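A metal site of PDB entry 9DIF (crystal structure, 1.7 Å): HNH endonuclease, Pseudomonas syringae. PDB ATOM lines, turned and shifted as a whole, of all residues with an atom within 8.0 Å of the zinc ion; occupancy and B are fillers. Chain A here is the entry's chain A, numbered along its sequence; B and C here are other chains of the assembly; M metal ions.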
ATOM      1  N   HIS A  31      11.357   6.791  32.047  1.00  0.00           N
ATOM      2  CA  HIS A  31       9.973   6.825  32.501  1.00  0.00           C
ATOM      3  C   HIS A  31       9.224   8.021  31.944  1.00  0.00           C
ATOM      4  O   HIS A  31       9.808   9.089  31.695  1.00  0.00           O
ATOM      5  CB  HIS A  31       9.863   6.871  34.047  1.00  0.00           C
ATOM      6  CG  HIS A  31      10.189   5.572  34.754  1.00  0.00           C
ATOM      7  ND1 HIS A  31      11.414   4.978  34.671  1.00  0.00           N
ATOM      8  CD2 HIS A  31       9.428   4.786  35.549  1.00  0.00           C
ATOM      9  CE1 HIS A  31      11.423   3.873  35.418  1.00  0.00           C
ATOM     10  NE2 HIS A  31      10.235   3.734  35.944  1.00  0.00           N
ATOM     11  N   CYS A  32       7.911   7.866  31.817  1.00  0.00           N
ATOM     12  CA  CYS A  32       7.096   8.979  31.329  1.00  0.00           C
ATOM     13  C   CYS A  32       7.129  10.121  32.346  1.00  0.00           C
ATOM     14  O   CYS A  32       6.750   9.958  33.515  1.00  0.00           O
ATOM     15  CB  CYS A  32       5.641   8.582  31.039  1.00  0.00           C
ATOM     16  SG  CYS A  32       4.587   9.906  30.488  1.00  0.00           S
ATOM     17  N   GLU A  33       7.448  11.321  31.858  1.00  0.00           N
ATOM     18  CA  GLU A  33       7.594  12.472  32.738  1.00  0.00           C
ATOM     19  C   GLU A  33       6.280  12.969  33.305  1.00  0.00           C
ATOM     20  O   GLU A  33       6.328  13.708  34.280  1.00  0.00           O
ATOM     21  CB  GLU A  33       8.282  13.628  32.028  1.00  0.00           C
ATOM     22  CG  GLU A  33       9.723  13.332  31.597  1.00  0.00           C
ATOM     23  CD  GLU A  33      10.420  14.551  31.022  1.00  0.00           C
ATOM     24  OE1 GLU A  33      10.285  15.575  31.689  1.00  0.00           O
ATOM     25  OE2 GLU A  33      11.094  14.517  29.977  1.00  0.00           O
ATOM     26  N   LEU A  34       5.133  12.622  32.694  1.00  0.00           N
ATOM     27  CA  LEU A  34       3.821  13.039  33.103  1.00  0.00           C
ATOM     28  C   LEU A  34       3.052  11.968  33.899  1.00  0.00           C
ATOM     29  O   LEU A  34       2.196  12.334  34.692  1.00  0.00           O
ATOM     30  CB  LEU A  34       3.012  13.481  31.874  1.00  0.00           C
ATOM     31  CG  LEU A  34       3.438  14.821  31.279  1.00  0.00           C
ATOM     32  CD1 LEU A  34       2.685  15.124  30.020  1.00  0.00           C
ATOM     33  CD2 LEU A  34       3.150  16.006  32.277  1.00  0.00           C
ATOM     34  N   CYS A  35       3.374  10.660  33.784  1.00  0.00           N
ATOM     35  CA  CYS A  35       2.619   9.667  34.560  1.00  0.00           C
ATOM     36  C   CYS A  35       3.517   8.644  35.263  1.00  0.00           C
ATOM     37  O   CYS A  35       3.005   7.868  36.083  1.00  0.00           O
ATOM     38  CB  CYS A  35       1.549   8.949  33.685  1.00  0.00           C
ATOM     39  SG  CYS A  35       2.310   7.750  32.510  1.00  0.00           S
ATOM     40  N   GLY A  36       4.815   8.623  34.992  1.00  0.00           N
ATOM     41  CA  GLY A  36       5.683   7.803  35.780  1.00  0.00           C
ATOM     42  C   GLY A  36       5.773   6.377  35.319  1.00  0.00           C
ATOM     43  O   GLY A  36       6.515   5.623  35.931  1.00  0.00           O
ATOM     44  N   THR A  37       5.089   5.990  34.234  1.00  0.00           N
ATOM     45  CA  THR A  37       5.166   4.595  33.820  1.00  0.00           C
ATOM     46  C   THR A  37       6.565   4.289  33.270  1.00  0.00           C
ATOM     47  O   THR A  37       7.234   5.148  32.713  1.00  0.00           O
ATOM     48  CB  THR A  37       4.059   4.297  32.806  1.00  0.00           C
ATOM     49  OG1 THR A  37       3.960   2.878  32.616  1.00  0.00           O
ATOM     50  CG2 THR A  37       4.407   4.888  31.428  1.00  0.00           C
ATOM     51  N   ASP A  38       7.014   3.043  33.437  1.00  0.00           N
ATOM     52  CA  ASP A  38       8.307   2.596  32.930  1.00  0.00           C
ATOM     53  C   ASP A  38       8.205   2.321  31.430  1.00  0.00           C
ATOM     54  O   ASP A  38       7.397   1.496  31.001  1.00  0.00           O
ATOM     55  CB  ASP A  38       8.697   1.327  33.672  1.00  0.00           C
ATOM     56  CG  ASP A  38      10.042   0.764  33.234  1.00  0.00           C
ATOM     57  OD1 ASP A  38      10.752   1.253  32.331  1.00  0.00           O
ATOM     58  OD2 ASP A  38      10.413  -0.222  33.893  1.00  0.00           O
ATOM     59  N   LEU A  39       9.006   3.022  30.646  1.00  0.00           N
ATOM     60  CA  LEU A  39       8.985   2.856  29.194  1.00  0.00           C
ATOM     61  C   LEU A  39      10.143   2.014  28.670  1.00  0.00           C
ATOM     62  O   LEU A  39      10.386   2.014  27.458  1.00  0.00           O
ATOM     63  CB  LEU A  39       9.008   4.213  28.540  1.00  0.00           C
ATOM     64  CG  LEU A  39       7.941   5.170  29.011  1.00  0.00           C
ATOM     65  CD1 LEU A  39       8.294   6.625  28.606  1.00  0.00           C
ATOM     66  CD2 LEU A  39       6.590   4.834  28.487  1.00  0.00           C
ATOM     67  N   TRP A  51       9.382   1.846  24.525  1.00  0.00           N
ATOM     68  CA  TRP A  51       8.072   2.137  23.935  1.00  0.00           C
ATOM     69  C   TRP A  51       7.620   3.586  24.190  1.00  0.00           C
ATOM     70  O   TRP A  51       6.427   3.904  24.042  1.00  0.00           O
ATOM     71  CB  TRP A  51       7.013   1.096  24.386  1.00  0.00           C
ATOM     72  CG  TRP A  51       6.677   0.981  25.865  1.00  0.00           C
ATOM     73  CD1 TRP A  51       7.429   0.319  26.800  1.00  0.00           C
ATOM     74  CD2 TRP A  51       5.519   1.502  26.574  1.00  0.00           C
ATOM     75  NE1 TRP A  51       6.803   0.354  28.027  1.00  0.00           N
ATOM     76  CE2 TRP A  51       5.643   1.098  27.920  1.00  0.00           C
ATOM     77  CE3 TRP A  51       4.375   2.253  26.186  1.00  0.00           C
ATOM     78  CZ2 TRP A  51       4.695   1.450  28.888  1.00  0.00           C
ATOM     79  CZ3 TRP A  51       3.453   2.598  27.126  1.00  0.00           C
ATOM     80  CH2 TRP A  51       3.600   2.194  28.457  1.00  0.00           C
ATOM     81  N   LEU A  85      10.406  12.969  27.494  1.00  0.00           N
ATOM     82  CA  LEU A  85      10.082  11.545  27.319  1.00  0.00           C
ATOM     83  C   LEU A  85       8.686  11.285  27.845  1.00  0.00           C
ATOM     84  O   LEU A  85       8.423  11.417  29.053  1.00  0.00           O
ATOM     85  CB  LEU A  85      11.074  10.624  28.050  1.00  0.00           C
ATOM     86  CG  LEU A  85      10.876   9.161  27.568  1.00  0.00           C
ATOM     87  CD1 LEU A  85      11.298   8.989  26.040  1.00  0.00           C
ATOM     88  CD2 LEU A  85      11.547   8.252  28.495  1.00  0.00           C
ATOM     89  N   LEU A  86       7.771  10.884  26.951  1.00  0.00           N
ATOM     90  CA  LEU A  86       6.373  10.614  27.262  1.00  0.00           C
ATOM     91  C   LEU A  86       5.954   9.227  26.772  1.00  0.00           C
ATOM     92  O   LEU A  86       6.388   8.763  25.717  1.00  0.00           O
ATOM     93  CB  LEU A  86       5.432  11.689  26.624  1.00  0.00           C
ATOM     94  CG  LEU A  86       5.725  13.146  26.992  1.00  0.00           C
ATOM     95  CD1 LEU A  86       4.774  14.037  26.232  1.00  0.00           C
ATOM     96  CD2 LEU A  86       5.521  13.279  28.482  1.00  0.00           C
ATOM     97  N   CYS A  87       5.058   8.584  27.525  1.00  0.00           N
ATOM     98  CA  CYS A  87       4.336   7.456  26.925  1.00  0.00           C
ATOM     99  C   CYS A  87       3.474   7.886  25.733  1.00  0.00           C
ATOM    100  O   CYS A  87       3.074   9.059  25.603  1.00  0.00           O
ATOM    101  CB  CYS A  87       3.485   6.743  27.992  1.00  0.00           C
ATOM    102  SG  CYS A  87       2.041   7.527  28.565  1.00  0.00           S
ATOM    103  N   PRO A  88       3.148   6.958  24.819  1.00  0.00           N
ATOM    104  CA  PRO A  88       2.360   7.368  23.652  1.00  0.00           C
ATOM    105  C   PRO A  88       1.004   7.990  24.005  1.00  0.00           C
ATOM    106  O   PRO A  88       0.443   8.829  23.281  1.00  0.00           O
ATOM    107  CB  PRO A  88       2.242   6.040  22.884  1.00  0.00           C
ATOM    108  CG  PRO A  88       3.438   5.197  23.369  1.00  0.00           C
ATOM    109  CD  PRO A  88       3.603   5.540  24.743  1.00  0.00           C
ATOM    110  N   GLY A  89       0.447   7.577  25.128  1.00  0.00           N
ATOM    111  CA  GLY A  89      -0.853   8.072  25.517  1.00  0.00           C
ATOM    112  C   GLY A  89      -0.793   9.489  26.058  1.00  0.00           C
ATOM    113  O   GLY A  89      -1.607  10.340  25.664  1.00  0.00           O
ATOM    114  N   CYS A  90       0.124   9.760  26.994  1.00  0.00           N
ATOM    115  CA  CYS A  90       0.311  11.131  27.471  1.00  0.00           C
ATOM    116  C   CYS A  90       0.661  12.038  26.312  1.00  0.00           C
ATOM    117  O   CYS A  90       0.137  13.144  26.196  1.00  0.00           O
ATOM    118  CB  CYS A  90       1.397  11.188  28.558  1.00  0.00           C
ATOM    119  SG  CYS A  90       0.810  10.432  30.140  1.00  0.00           S
ATOM    120  N   HIS A  91       1.482  11.556  25.396  1.00  0.00           N
ATOM    121  CA  HIS A  91       1.880  12.390  24.273  1.00  0.00           C
ATOM    122  C   HIS A  91       0.685  12.738  23.387  1.00  0.00           C
ATOM    123  O   HIS A  91       0.521  13.871  22.926  1.00  0.00           O
ATOM    124  CB  HIS A  91       2.958  11.678  23.473  1.00  0.00           C
ATOM    125  CG  HIS A  91       3.609  12.553  22.448  1.00  0.00           C
ATOM    126  ND1 HIS A  91       4.314  12.066  21.373  1.00  0.00           N
ATOM    127  CD2 HIS A  91       3.653  13.899  22.350  1.00  0.00           C
ATOM    128  CE1 HIS A  91       4.778  13.082  20.664  1.00  0.00           C
ATOM    129  NE2 HIS A  91       4.371  14.197  21.230  1.00  0.00           N
ATOM    130  N   LYS A  93      -2.434  12.918  24.252  1.00  0.00           N
ATOM    131  CA  LYS A  93      -3.369  13.856  24.881  1.00  0.00           C
ATOM    132  C   LYS A  93      -2.853  15.300  24.909  1.00  0.00           C
ATOM    133  O   LYS A  93      -3.645  16.220  24.698  1.00  0.00           O
ATOM    134  CB  LYS A  93      -3.633  13.386  26.300  1.00  0.00           C
ATOM    135  CG  LYS A  93      -4.472  12.116  26.421  1.00  0.00           C
ATOM    136  CD  LYS A  93      -4.137  11.526  27.904  1.00  0.00           C
ATOM    137  CE  LYS A  93      -4.897  10.256  28.152  1.00  0.00           C
ATOM    138  NZ  LYS A  93      -4.518   9.667  29.465  1.00  0.00           N
ATOM    139  N   ARG B  44      -7.425  13.965  32.982  1.00  0.00           N
ATOM    140  CA  ARG B  44      -6.465  14.795  33.654  1.00  0.00           C
ATOM    141  C   ARG B  44      -6.775  16.260  33.482  1.00  0.00           C
ATOM    142  O   ARG B  44      -6.587  17.053  34.400  1.00  0.00           O
ATOM    143  CB  ARG B  44      -5.070  14.458  33.138  1.00  0.00           C
ATOM    144  CG  ARG B  44      -3.971  15.303  33.712  1.00  0.00           C
ATOM    145  CD  ARG B  44      -2.572  14.997  33.268  1.00  0.00           C
ATOM    146  NE  ARG B  44      -1.607  15.971  33.776  1.00  0.00           N
ATOM    147  CZ  ARG B  44      -0.406  15.658  34.257  1.00  0.00           C
ATOM    148  NH1 ARG B  44       0.083  14.417  34.170  1.00  0.00           N
ATOM    149  NH2 ARG B  44       0.304  16.598  34.892  1.00  0.00           N
ATOM    150  N   PRO C 124       5.625  10.944  39.423  1.00  0.00           N
ATOM    151  CA  PRO C 124       4.377  11.438  38.826  1.00  0.00           C
ATOM    152  C   PRO C 124       3.152  10.586  39.132  1.00  0.00           C
ATOM    153  O   PRO C 124       2.037  11.119  39.069  1.00  0.00           O
ATOM    154  CB  PRO C 124       4.697  11.468  37.322  1.00  0.00           C
ATOM    155  CG  PRO C 124       6.295  11.643  37.307  1.00  0.00           C
ATOM    156  CD  PRO C 124       6.758  10.934  38.473  1.00  0.00           C
HETATM  157 ZN    ZN M   1       2.495   8.838  30.459  1.00  0.00          ZN
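The backbone NH (N) of Leu 34 sits close to the side-chain sulfur (SG) of Cys 32 (3.5 Å).
The backbone NH (N) of Thr 37 sits close to the side-chain sulfur (SG) of Cys 35, at 3.7 Å.
N of Cys 32 sits at hydrogen-bond distance from O of Thr 37 (2.9 Å).
N of Gly 89 sits close to SG of Cys 87.
Within 4 Å of the zinc ion: Cys 32, Cys 35, Cys 87 and Cys 90.
The nearest printed residue that does not touch the zinc ion is Thr 37 (4.5 Å).
The zinc ion is bound by SG of Cys 35, SG of Cys 90, SG of Cys 87 and SG of Cys 32.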
